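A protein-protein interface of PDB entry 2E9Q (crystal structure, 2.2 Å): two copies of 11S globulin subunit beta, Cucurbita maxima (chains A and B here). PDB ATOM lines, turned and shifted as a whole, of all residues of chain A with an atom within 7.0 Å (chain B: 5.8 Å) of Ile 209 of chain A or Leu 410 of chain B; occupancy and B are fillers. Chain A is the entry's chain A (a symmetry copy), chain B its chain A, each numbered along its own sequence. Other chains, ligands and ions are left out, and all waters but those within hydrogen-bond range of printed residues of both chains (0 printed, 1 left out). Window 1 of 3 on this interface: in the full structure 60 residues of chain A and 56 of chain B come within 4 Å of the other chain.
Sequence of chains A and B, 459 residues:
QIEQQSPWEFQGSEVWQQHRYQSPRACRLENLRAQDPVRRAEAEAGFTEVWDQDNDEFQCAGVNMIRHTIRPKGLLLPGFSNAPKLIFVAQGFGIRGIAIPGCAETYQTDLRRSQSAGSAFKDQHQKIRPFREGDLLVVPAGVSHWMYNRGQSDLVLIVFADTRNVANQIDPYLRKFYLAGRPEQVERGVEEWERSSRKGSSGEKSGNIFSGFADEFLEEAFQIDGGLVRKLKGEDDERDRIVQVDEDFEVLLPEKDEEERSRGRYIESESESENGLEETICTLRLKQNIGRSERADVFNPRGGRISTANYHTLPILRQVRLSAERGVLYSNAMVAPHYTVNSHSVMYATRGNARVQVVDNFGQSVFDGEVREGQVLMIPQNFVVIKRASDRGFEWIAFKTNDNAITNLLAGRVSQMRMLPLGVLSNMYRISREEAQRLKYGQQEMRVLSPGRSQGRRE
The backbone NH of Gly 212 of chain A sits close to the backbone carbonyl oxygen of Gly 363 of chain B, 3.3 Å away.
The backbone NH (N) of Asn 408 of chain B sits at hydrogen-bond distance from the backbone carbonyl oxygen (O) of Tyr 339 of chain B.
The side-chain carboxylate (OD2) of Asp 360 of chain B is in hydrogen-bond range of the backbone NH (N) of Gly 363 of chain B (3.0 Å).
O of Leu 409 of chain B is in hydrogen-bond range of N of Gln 416 of chain B.
The backbone NH (N) of Met 417 of chain B lies close to the backbone carbonyl oxygen (O) of Leu 410 of chain B (3.5 Å).
The backbone carbonyl oxygen (O) of Phe 80 of chain A sits at hydrogen-bond distance from the backbone NH (N) of Phe 177 of chain A (2.6 Å).
The side-chain hydroxyl (OG) of Ser 211 of chain A lies within hydrogen-bond range of the backbone carbonyl oxygen (O) of Asn 208 of chain A.
Phe 80 of chain A touches Tyr 339 of chain B.
Lys 176 of chain A touches Asn 361 of chain B (O to O, 3.5 Å).
Asp 360 of chain B touches Phe 177 of chain A (C to CE2, 3.6 Å).
Gly 207 of chain A touches Gly 363 of chain B (O to N, 3.7 Å).
Gly 363 of chain B touches Asn 208 of chain A.
Val 384 of chain B touches Ile 209 of chain A.
Leu 410 of chain B touches Ile 209 of chain A.
Ser 211 of chain A touches Gly 363 of chain B.
Phe 213 of chain A touches Val 384 of chain B (CE2 to CG1, 3.4 Å).
Ala 411 of chain B touches Phe 222 of chain A.
Ile 209 of chain A touches just these residues of chain B: Val 359, Val 384 and Leu 410.
Pro 337 of chain B touches none of the printed residues of chain A.
His 338 of chain B touches none of the printed residues of chain A.
Of the printed residues of chain A, Tyr 339 of chain B touches Phe 80.
Of the printed residues of chain A, Val 359 of chain B touches Ile 209 (3.4 Å), Gly 212 (3.4 Å) and Phe 213 (3.5 Å).
Printed residues of chain A within 4 Å of Leu 410 of chain B: Ile 209.
The nearest residue of chain B that does not touch Ile 209 of chain A is Asp 360 of chain B (4.4 Å).
The nearest residue of chain A that does not touch Leu 410 of chain B is Phe 210 of chain A (4.1 Å).
The nearest printed residue of chain A that does not touch Gln 416 of chain B is Phe 80 of chain A (6.2 Å).
Printed residues of chain A that touch a printed residue of chain B: Phe 80, Lys 176, Phe 177, Leu 179, Gly 207, Asn 208, Ile 209, Ser 211, Gly 212, Phe 213 and Phe 222.
Hydrophobic or aromatic side chains of chain A that line the printed part of chain B: Phe 80, Phe 177, Leu 179, Ile 209, Phe 213 and Phe 222.
Printed residues of chain B that touch a printed residue of chain A: Tyr 339, Val 359, Asp 360, Asn 361, Gly 363, Val 384, Leu 410, Ala 411 and Gln 416.
Hydrophobic or aromatic side chains of chain B within 4 Å of the printed part of chain A: Tyr 339, Val 359, Val 384, Leu 410 and Ala 411.
Among the printed residues, 16 pairs touch across the chains.
Among the printed residues, no Asp or Glu carboxylate lies within 4 Å of a Lys or Arg side-chain nitrogen of the other chain.
No position is printed for both chains.
Of the 16 pairs that touch across the chains among the printed residues, none has its exchanged pair printed and touching as well.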
ATOM      1  N   PHE A  80      -3.474   1.310 -24.735  1.00  0.00           N
ATOM      2  CA  PHE A  80      -4.750   1.979 -24.968  1.00  0.00           C
ATOM      3  C   PHE A  80      -5.003   2.938 -23.819  1.00  0.00           C
ATOM      4  O   PHE A  80      -4.503   2.725 -22.721  1.00  0.00           O
ATOM      5  CB  PHE A  80      -5.907   0.969 -25.084  1.00  0.00           C
ATOM      6  CG  PHE A  80      -6.019   0.008 -23.933  1.00  0.00           C
ATOM      7  CD1 PHE A  80      -5.253  -1.152 -23.897  1.00  0.00           C
ATOM      8  CD2 PHE A  80      -6.917   0.244 -22.894  1.00  0.00           C
ATOM      9  CE1 PHE A  80      -5.379  -2.066 -22.850  1.00  0.00           C
ATOM     10  CE2 PHE A  80      -7.048  -0.662 -21.846  1.00  0.00           C
ATOM     11  CZ  PHE A  80      -6.279  -1.818 -21.824  1.00  0.00           C
ATOM     12  N   LYS A 176      -2.815   5.525 -19.626  1.00  0.00           N
ATOM     13  CA  LYS A 176      -2.494   4.698 -20.775  1.00  0.00           C
ATOM     14  C   LYS A 176      -2.075   3.308 -20.309  1.00  0.00           C
ATOM     15  O   LYS A 176      -1.135   3.153 -19.532  1.00  0.00           O
ATOM     16  CB  LYS A 176      -1.411   5.334 -21.657  1.00  0.00           C
ATOM     17  CG  LYS A 176      -1.259   4.573 -22.972  1.00  0.00           C
ATOM     18  CD  LYS A 176      -0.451   5.282 -24.031  1.00  0.00           C
ATOM     19  CE  LYS A 176      -0.179   4.315 -25.190  1.00  0.00           C
ATOM     20  NZ  LYS A 176       0.625   4.914 -26.270  1.00  0.00           N
ATOM     21  N   PHE A 177      -2.811   2.303 -20.774  1.00  0.00           N
ATOM     22  CA  PHE A 177      -2.576   0.898 -20.433  1.00  0.00           C
ATOM     23  C   PHE A 177      -1.709   0.222 -21.499  1.00  0.00           C
ATOM     24  O   PHE A 177      -2.170  -0.031 -22.619  1.00  0.00           O
ATOM     25  CB  PHE A 177      -3.913   0.137 -20.328  1.00  0.00           C
ATOM     26  CG  PHE A 177      -4.887   0.730 -19.342  1.00  0.00           C
ATOM     27  CD1 PHE A 177      -5.496   1.956 -19.593  1.00  0.00           C
ATOM     28  CD2 PHE A 177      -5.179   0.072 -18.156  1.00  0.00           C
ATOM     29  CE1 PHE A 177      -6.385   2.522 -18.667  1.00  0.00           C
ATOM     30  CE2 PHE A 177      -6.070   0.634 -17.221  1.00  0.00           C
ATOM     31  CZ  PHE A 177      -6.667   1.859 -17.485  1.00  0.00           C
ATOM     32  N   TYR A 178      -0.467  -0.083 -21.142  1.00  0.00           N
ATOM     33  CA  TYR A 178       0.466  -0.725 -22.058  1.00  0.00           C
ATOM     34  C   TYR A 178       0.378  -2.242 -21.996  1.00  0.00           C
ATOM     35  O   TYR A 178       0.274  -2.824 -20.912  1.00  0.00           O
ATOM     36  CB  TYR A 178       1.910  -0.281 -21.756  1.00  0.00           C
ATOM     37  CG  TYR A 178       2.257   1.063 -22.339  1.00  0.00           C
ATOM     38  CD1 TYR A 178       2.046   2.249 -21.628  1.00  0.00           C
ATOM     39  CD2 TYR A 178       2.753   1.156 -23.635  1.00  0.00           C
ATOM     40  CE1 TYR A 178       2.323   3.497 -22.209  1.00  0.00           C
ATOM     41  CE2 TYR A 178       3.028   2.385 -24.221  1.00  0.00           C
ATOM     42  CZ  TYR A 178       2.814   3.548 -23.511  1.00  0.00           C
ATOM     43  OH  TYR A 178       3.096   4.740 -24.140  1.00  0.00           O
ATOM     44  N   LEU A 179       0.417  -2.880 -23.162  1.00  0.00           N
ATOM     45  CA  LEU A 179       0.351  -4.338 -23.226  1.00  0.00           C
ATOM     46  C   LEU A 179       1.720  -4.990 -23.026  1.00  0.00           C
ATOM     47  O   LEU A 179       1.802  -6.155 -22.643  1.00  0.00           O
ATOM     48  CB  LEU A 179      -0.228  -4.797 -24.565  1.00  0.00           C
ATOM     49  CG  LEU A 179      -1.610  -4.287 -25.002  1.00  0.00           C
ATOM     50  CD1 LEU A 179      -2.157  -5.226 -26.066  1.00  0.00           C
ATOM     51  CD2 LEU A 179      -2.560  -4.236 -23.834  1.00  0.00           C
ATOM     52  N   ALA A 180       2.791  -4.244 -23.285  1.00  0.00           N
ATOM     53  CA  ALA A 180       4.142  -4.788 -23.123  1.00  0.00           C
ATOM     54  C   ALA A 180       5.137  -3.771 -22.587  1.00  0.00           C
ATOM     55  O   ALA A 180       4.860  -2.573 -22.553  1.00  0.00           O
ATOM     56  CB  ALA A 180       4.647  -5.331 -24.444  1.00  0.00           C
ATOM     57  N   GLY A 181       6.308  -4.264 -22.183  1.00  0.00           N
ATOM     58  CA  GLY A 181       7.350  -3.391 -21.668  1.00  0.00           C
ATOM     59  C   GLY A 181       7.092  -2.894 -20.261  1.00  0.00           C
ATOM     60  O   GLY A 181       6.215  -3.387 -19.565  1.00  0.00           O
ATOM     61  N   GLY A 207       4.238  -0.835 -14.348  1.00  0.00           N
ATOM     62  CA  GLY A 207       4.516  -1.750 -15.435  1.00  0.00           C
ATOM     63  C   GLY A 207       3.398  -1.838 -16.456  1.00  0.00           C
ATOM     64  O   GLY A 207       2.570  -0.945 -16.555  1.00  0.00           O
ATOM     65  N   ASN A 208       3.387  -2.918 -17.226  1.00  0.00           N
ATOM     66  CA  ASN A 208       2.362  -3.126 -18.242  1.00  0.00           C
ATOM     67  C   ASN A 208       1.183  -3.826 -17.563  1.00  0.00           C
ATOM     68  O   ASN A 208       1.305  -4.264 -16.423  1.00  0.00           O
ATOM     69  CB  ASN A 208       2.929  -3.972 -19.390  1.00  0.00           C
ATOM     70  CG  ASN A 208       3.409  -5.335 -18.929  1.00  0.00           C
ATOM     71  OD1 ASN A 208       2.700  -6.052 -18.216  1.00  0.00           O
ATOM     72  ND2 ASN A 208       4.616  -5.704 -19.340  1.00  0.00           N
ATOM     73  N   ILE A 209       0.054  -3.953 -18.254  1.00  0.00           N
ATOM     74  CA  ILE A 209      -1.128  -4.578 -17.644  1.00  0.00           C
ATOM     75  C   ILE A 209      -0.978  -6.007 -17.142  1.00  0.00           C
ATOM     76  O   ILE A 209      -1.737  -6.437 -16.276  1.00  0.00           O
ATOM     77  CB  ILE A 209      -2.330  -4.570 -18.600  1.00  0.00           C
ATOM     78  CG1 ILE A 209      -1.996  -5.392 -19.854  1.00  0.00           C
ATOM     79  CG2 ILE A 209      -2.713  -3.132 -18.919  1.00  0.00           C
ATOM     80  CD1 ILE A 209      -3.121  -5.495 -20.847  1.00  0.00           C
ATOM     81  N   PHE A 210      -0.016  -6.751 -17.674  1.00  0.00           N
ATOM     82  CA  PHE A 210       0.154  -8.131 -17.233  1.00  0.00           C
ATOM     83  C   PHE A 210       0.951  -8.257 -15.945  1.00  0.00           C
ATOM     84  O   PHE A 210       0.744  -9.197 -15.188  1.00  0.00           O
ATOM     85  CB  PHE A 210       0.811  -8.970 -18.338  1.00  0.00           C
ATOM     86  CG  PHE A 210       0.001  -9.035 -19.589  1.00  0.00           C
ATOM     87  CD1 PHE A 210       0.456  -8.449 -20.760  1.00  0.00           C
ATOM     88  CD2 PHE A 210      -1.268  -9.616 -19.579  1.00  0.00           C
ATOM     89  CE1 PHE A 210      -0.340  -8.430 -21.907  1.00  0.00           C
ATOM     90  CE2 PHE A 210      -2.071  -9.601 -20.723  1.00  0.00           C
ATOM     91  CZ  PHE A 210      -1.604  -9.003 -21.885  1.00  0.00           C
ATOM     92  N   SER A 211       1.847  -7.308 -15.680  1.00  0.00           N
ATOM     93  CA  SER A 211       2.660  -7.389 -14.469  1.00  0.00           C
ATOM     94  C   SER A 211       1.857  -7.290 -13.188  1.00  0.00           C
ATOM     95  O   SER A 211       2.384  -7.544 -12.108  1.00  0.00           O
ATOM     96  CB  SER A 211       3.786  -6.342 -14.476  1.00  0.00           C
ATOM     97  OG  SER A 211       3.303  -5.017 -14.492  1.00  0.00           O
ATOM     98  N   GLY A 212       0.578  -6.949 -13.300  1.00  0.00           N
ATOM     99  CA  GLY A 212      -0.256  -6.860 -12.114  1.00  0.00           C
ATOM    100  C   GLY A 212      -1.009  -8.143 -11.782  1.00  0.00           C
ATOM    101  O   GLY A 212      -1.636  -8.234 -10.729  1.00  0.00           O
ATOM    102  N   PHE A 213      -0.953  -9.140 -12.664  1.00  0.00           N
ATOM    103  CA  PHE A 213      -1.649 -10.415 -12.428  1.00  0.00           C
ATOM    104  C   PHE A 213      -0.729 -11.521 -11.903  1.00  0.00           C
ATOM    105  O   PHE A 213       0.469 -11.542 -12.193  1.00  0.00           O
ATOM    106  CB  PHE A 213      -2.313 -10.922 -13.721  1.00  0.00           C
ATOM    107  CG  PHE A 213      -3.542 -10.152 -14.125  1.00  0.00           C
ATOM    108  CD1 PHE A 213      -4.721 -10.256 -13.396  1.00  0.00           C
ATOM    109  CD2 PHE A 213      -3.517  -9.314 -15.238  1.00  0.00           C
ATOM    110  CE1 PHE A 213      -5.853  -9.540 -13.763  1.00  0.00           C
ATOM    111  CE2 PHE A 213      -4.654  -8.593 -15.613  1.00  0.00           C
ATOM    112  CZ  PHE A 213      -5.816  -8.708 -14.875  1.00  0.00           C
ATOM    113  N   LEU A 218      -2.148 -16.003 -15.567  1.00  0.00           N
ATOM    114  CA  LEU A 218      -1.638 -15.796 -16.910  1.00  0.00           C
ATOM    115  C   LEU A 218      -1.205 -17.087 -17.600  1.00  0.00           C
ATOM    116  O   LEU A 218      -1.219 -17.173 -18.830  1.00  0.00           O
ATOM    117  CB  LEU A 218      -0.493 -14.781 -16.889  1.00  0.00           C
ATOM    118  CG  LEU A 218      -0.914 -13.390 -16.395  1.00  0.00           C
ATOM    119  CD1 LEU A 218       0.250 -12.427 -16.519  1.00  0.00           C
ATOM    120  CD2 LEU A 218      -2.103 -12.891 -17.202  1.00  0.00           C
ATOM    121  N   PHE A 222      -3.274 -17.766 -20.991  1.00  0.00           N
ATOM    122  CA  PHE A 222      -2.605 -17.914 -22.280  1.00  0.00           C
ATOM    123  C   PHE A 222      -2.122 -19.328 -22.588  1.00  0.00           C
ATOM    124  O   PHE A 222      -1.647 -19.588 -23.691  1.00  0.00           O
ATOM    125  CB  PHE A 222      -1.406 -16.970 -22.377  1.00  0.00           C
ATOM    126  CG  PHE A 222      -1.763 -15.522 -22.320  1.00  0.00           C
ATOM    127  CD1 PHE A 222      -2.188 -14.943 -21.133  1.00  0.00           C
ATOM    128  CD2 PHE A 222      -1.650 -14.722 -23.454  1.00  0.00           C
ATOM    129  CE1 PHE A 222      -2.490 -13.594 -21.074  1.00  0.00           C
ATOM    130  CE2 PHE A 222      -1.953 -13.364 -23.404  1.00  0.00           C
ATOM    131  CZ  PHE A 222      -2.372 -12.800 -22.211  1.00  0.00           C
ATOM    132  N   PRO B 337      -8.714 -12.754 -19.415  1.00  0.00           N
ATOM    133  CA  PRO B 337      -8.384 -11.363 -19.102  1.00  0.00           C
ATOM    134  C   PRO B 337      -8.988 -10.470 -20.175  1.00  0.00           C
ATOM    135  O   PRO B 337      -8.886 -10.748 -21.368  1.00  0.00           O
ATOM    136  CB  PRO B 337      -6.852 -11.346 -19.116  1.00  0.00           C
ATOM    137  CG  PRO B 337      -6.476 -12.565 -19.926  1.00  0.00           C
ATOM    138  CD  PRO B 337      -7.491 -13.574 -19.481  1.00  0.00           C
ATOM    139  N   HIS B 338      -9.618  -9.392 -19.739  1.00  0.00           N
ATOM    140  CA  HIS B 338     -10.253  -8.483 -20.672  1.00  0.00           C
ATOM    141  C   HIS B 338     -10.568  -7.176 -19.955  1.00  0.00           C
ATOM    142  O   HIS B 338     -10.446  -7.071 -18.739  1.00  0.00           O
ATOM    143  CB  HIS B 338     -11.576  -9.080 -21.130  1.00  0.00           C
ATOM    144  CG  HIS B 338     -12.577  -9.178 -20.027  1.00  0.00           C
ATOM    145  ND1 HIS B 338     -12.581 -10.212 -19.120  1.00  0.00           N
ATOM    146  CD2 HIS B 338     -13.544  -8.319 -19.622  1.00  0.00           C
ATOM    147  CE1 HIS B 338     -13.506  -9.991 -18.203  1.00  0.00           C
ATOM    148  NE2 HIS B 338     -14.104  -8.849 -18.484  1.00  0.00           N
ATOM    149  N   TYR B 339     -10.998  -6.190 -20.724  1.00  0.00           N
ATOM    150  CA  TYR B 339     -11.383  -4.923 -20.155  1.00  0.00           C
ATOM    151  C   TYR B 339     -12.510  -4.376 -21.013  1.00  0.00           C
ATOM    152  O   TYR B 339     -12.660  -4.757 -22.173  1.00  0.00           O
ATOM    153  CB  TYR B 339     -10.197  -3.954 -20.139  1.00  0.00           C
ATOM    154  CG  TYR B 339      -9.708  -3.562 -21.505  1.00  0.00           C
ATOM    155  CD1 TYR B 339      -8.791  -4.353 -22.206  1.00  0.00           C
ATOM    156  CD2 TYR B 339     -10.145  -2.382 -22.091  1.00  0.00           C
ATOM    157  CE1 TYR B 339      -8.321  -3.959 -23.448  1.00  0.00           C
ATOM    158  CE2 TYR B 339      -9.691  -1.991 -23.314  1.00  0.00           C
ATOM    159  CZ  TYR B 339      -8.779  -2.768 -23.995  1.00  0.00           C
ATOM    160  OH  TYR B 339      -8.333  -2.314 -25.221  1.00  0.00           O
ATOM    161  N   VAL B 359      -6.330  -5.055 -12.685  1.00  0.00           N
ATOM    162  CA  VAL B 359      -5.091  -4.314 -12.825  1.00  0.00           C
ATOM    163  C   VAL B 359      -5.341  -2.967 -13.471  1.00  0.00           C
ATOM    164  O   VAL B 359      -6.200  -2.837 -14.350  1.00  0.00           O
ATOM    165  CB  VAL B 359      -4.068  -5.118 -13.666  1.00  0.00           C
ATOM    166  CG1 VAL B 359      -2.798  -4.317 -13.866  1.00  0.00           C
ATOM    167  CG2 VAL B 359      -3.753  -6.439 -12.970  1.00  0.00           C
ATOM    168  N   ASP B 360      -4.593  -1.956 -13.041  1.00  0.00           N
ATOM    169  CA  ASP B 360      -4.781  -0.625 -13.593  1.00  0.00           C
ATOM    170  C   ASP B 360      -3.730  -0.258 -14.621  1.00  0.00           C
ATOM    171  O   ASP B 360      -2.943  -1.103 -15.046  1.00  0.00           O
ATOM    172  CB  ASP B 360      -4.842   0.418 -12.468  1.00  0.00           C
ATOM    173  CG  ASP B 360      -3.513   0.584 -11.727  1.00  0.00           C
ATOM    174  OD1 ASP B 360      -3.550   1.202 -10.647  1.00  0.00           O
ATOM    175  OD2 ASP B 360      -2.448   0.124 -12.220  1.00  0.00           O
ATOM    176  N   ASN B 361      -3.744   1.002 -15.040  1.00  0.00           N
ATOM    177  CA  ASN B 361      -2.816   1.496 -16.049  1.00  0.00           C
ATOM    178  C   ASN B 361      -1.366   1.571 -15.574  1.00  0.00           C
ATOM    179  O   ASN B 361      -0.445   1.737 -16.384  1.00  0.00           O
ATOM    180  CB  ASN B 361      -3.281   2.867 -16.543  1.00  0.00           C
ATOM    181  CG  ASN B 361      -3.417   3.880 -15.415  1.00  0.00           C
ATOM    182  OD1 ASN B 361      -2.641   4.829 -15.321  1.00  0.00           O
ATOM    183  ND2 ASN B 361      -4.398   3.678 -14.558  1.00  0.00           N
ATOM    184  N   GLY B 363      -0.213  -0.843 -14.048  1.00  0.00           N
ATOM    185  CA  GLY B 363       0.108  -2.250 -14.021  1.00  0.00           C
ATOM    186  C   GLY B 363       0.030  -2.763 -12.603  1.00  0.00           C
ATOM    187  O   GLY B 363       0.576  -3.820 -12.297  1.00  0.00           O
ATOM    188  N   VAL B 384      -8.109  -3.883 -16.529  1.00  0.00           N
ATOM    189  CA  VAL B 384      -8.011  -5.276 -16.941  1.00  0.00           C
ATOM    190  C   VAL B 384      -8.451  -6.222 -15.840  1.00  0.00           C
ATOM    191  O   VAL B 384      -8.150  -6.008 -14.662  1.00  0.00           O
ATOM    192  CB  VAL B 384      -6.580  -5.597 -17.391  1.00  0.00           C
ATOM    193  CG1 VAL B 384      -6.511  -7.000 -17.944  1.00  0.00           C
ATOM    194  CG2 VAL B 384      -6.147  -4.581 -18.456  1.00  0.00           C
ATOM    195  N   ASN B 408     -12.862  -6.125 -24.751  1.00  0.00           N
ATOM    196  CA  ASN B 408     -11.732  -6.554 -25.558  1.00  0.00           C
ATOM    197  C   ASN B 408     -11.011  -7.657 -24.793  1.00  0.00           C
ATOM    198  O   ASN B 408     -10.687  -7.495 -23.611  1.00  0.00           O
ATOM    199  CB  ASN B 408     -10.758  -5.398 -25.802  1.00  0.00           C
ATOM    200  CG  ASN B 408     -11.112  -4.583 -27.016  1.00  0.00           C
ATOM    201  OD1 ASN B 408     -10.344  -3.721 -27.445  1.00  0.00           O
ATOM    202  ND2 ASN B 408     -12.284  -4.847 -27.583  1.00  0.00           N
ATOM    203  N   LEU B 409     -10.767  -8.778 -25.459  1.00  0.00           N
ATOM    204  CA  LEU B 409     -10.072  -9.886 -24.824  1.00  0.00           C
ATOM    205  C   LEU B 409      -8.577  -9.748 -25.049  1.00  0.00           C
ATOM    206  O   LEU B 409      -8.140  -9.259 -26.090  1.00  0.00           O
ATOM    207  CB  LEU B 409     -10.556 -11.219 -25.394  1.00  0.00           C
ATOM    208  CG  LEU B 409     -11.956 -11.665 -24.973  1.00  0.00           C
ATOM    209  CD1 LEU B 409     -12.991 -10.667 -25.468  1.00  0.00           C
ATOM    210  CD2 LEU B 409     -12.231 -13.050 -25.549  1.00  0.00           C
ATOM    211  N   LEU B 410      -7.791 -10.166 -24.067  1.00  0.00           N
ATOM    212  CA  LEU B 410      -6.346 -10.068 -24.203  1.00  0.00           C
ATOM    213  C   LEU B 410      -5.774 -11.291 -24.894  1.00  0.00           C
ATOM    214  O   LEU B 410      -4.794 -11.183 -25.632  1.00  0.00           O
ATOM    215  CB  LEU B 410      -5.675  -9.873 -22.838  1.00  0.00           C
ATOM    216  CG  LEU B 410      -5.753  -8.472 -22.223  1.00  0.00           C
ATOM    217  CD1 LEU B 410      -5.422  -7.438 -23.293  1.00  0.00           C
ATOM    218  CD2 LEU B 410      -7.135  -8.214 -21.667  1.00  0.00           C
ATOM    219  N   ALA B 411      -6.389 -12.445 -24.660  1.00  0.00           N
ATOM    220  CA  ALA B 411      -5.939 -13.692 -25.282  1.00  0.00           C
ATOM    221  C   ALA B 411      -7.132 -14.540 -25.732  1.00  0.00           C
ATOM    222  O   ALA B 411      -8.225 -14.414 -25.184  1.00  0.00           O
ATOM    223  CB  ALA B 411      -5.082 -14.475 -24.306  1.00  0.00           C
ATOM    224  N   GLY B 412      -6.922 -15.407 -26.722  1.00  0.00           N
ATOM    225  CA  GLY B 412      -8.005 -16.251 -27.210  1.00  0.00           C
ATOM    226  C   GLY B 412      -8.131 -16.170 -28.716  1.00  0.00           C
ATOM    227  O   GLY B 412      -7.267 -15.581 -29.358  1.00  0.00           O
ATOM    228  N   SER B 415      -8.652 -11.793 -30.210  1.00  0.00           N
ATOM    229  CA  SER B 415      -8.059 -10.978 -29.167  1.00  0.00           C
ATOM    230  C   SER B 415      -7.023  -9.985 -29.666  1.00  0.00           C
ATOM    231  O   SER B 415      -6.652  -9.975 -30.838  1.00  0.00           O
ATOM    232  CB  SER B 415      -7.428 -11.884 -28.107  1.00  0.00           C
ATOM    233  OG  SER B 415      -6.396 -12.668 -28.675  1.00  0.00           O
ATOM    234  N   GLN B 416      -6.567  -9.140 -28.749  1.00  0.00           N
ATOM    235  CA  GLN B 416      -5.572  -8.136 -29.065  1.00  0.00           C
ATOM    236  C   GLN B 416      -4.274  -8.830 -29.447  1.00  0.00           C
ATOM    237  O   GLN B 416      -3.588  -8.423 -30.377  1.00  0.00           O
ATOM    238  CB  GLN B 416      -5.345  -7.230 -27.847  1.00  0.00           C
ATOM    239  CG  GLN B 416      -5.515  -5.739 -28.130  1.00  0.00           C
ATOM    240  CD  GLN B 416      -6.945  -5.355 -28.491  1.00  0.00           C
ATOM    241  OE1 GLN B 416      -7.205  -4.220 -28.892  1.00  0.00           O
ATOM    242  NE2 GLN B 416      -7.876  -6.293 -28.348  1.00  0.00           N
ATOM    243  N   MET B 417      -3.949  -9.892 -28.728  1.00  0.00           N
ATOM    244  CA  MET B 417      -2.723 -10.631 -28.982  1.00  0.00           C
ATOM    245  C   MET B 417      -2.758 -11.221 -30.402  1.00  0.00           C
ATOM    246  O   MET B 417      -1.765 -11.176 -31.130  1.00  0.00           O
ATOM    247  CB  MET B 417      -2.543 -11.737 -27.939  1.00  0.00           C
ATOM    248  CG  MET B 417      -1.166 -11.752 -27.269  1.00  0.00           C
ATOM    249  SD  MET B 417      -0.853 -10.401 -26.091  1.00  0.00           S
ATOM    250  CE  MET B 417      -0.048  -9.193 -27.134  1.00  0.00           C
ATOM    251  N   ARG B 418      -3.913 -11.756 -30.793  1.00  0.00           N
ATOM    252  CA  ARG B 418      -4.089 -12.352 -32.115  1.00  0.00           C
ATOM    253  C   ARG B 418      -3.927 -11.329 -33.230  1.00  0.00           C
ATOM    254  O   ARG B 418      -3.380 -11.634 -34.287  1.00  0.00           O
ATOM    255  CB  ARG B 418      -5.477 -12.989 -32.220  1.00  0.00           C
ATOM    256  CG  ARG B 418      -5.704 -14.162 -31.279  1.00  0.00           C
ATOM    257  CD  ARG B 418      -5.548 -15.482 -32.006  1.00  0.00           C
ATOM    258  NE  ARG B 418      -5.810 -16.627 -31.139  1.00  0.00           N
ATOM    259  CZ  ARG B 418      -5.926 -17.879 -31.572  1.00  0.00           C
ATOM    260  NH1 ARG B 418      -5.807 -18.152 -32.863  1.00  0.00           N
ATOM    261  NH2 ARG B 418      -6.170 -18.857 -30.714  1.00  0.00           N
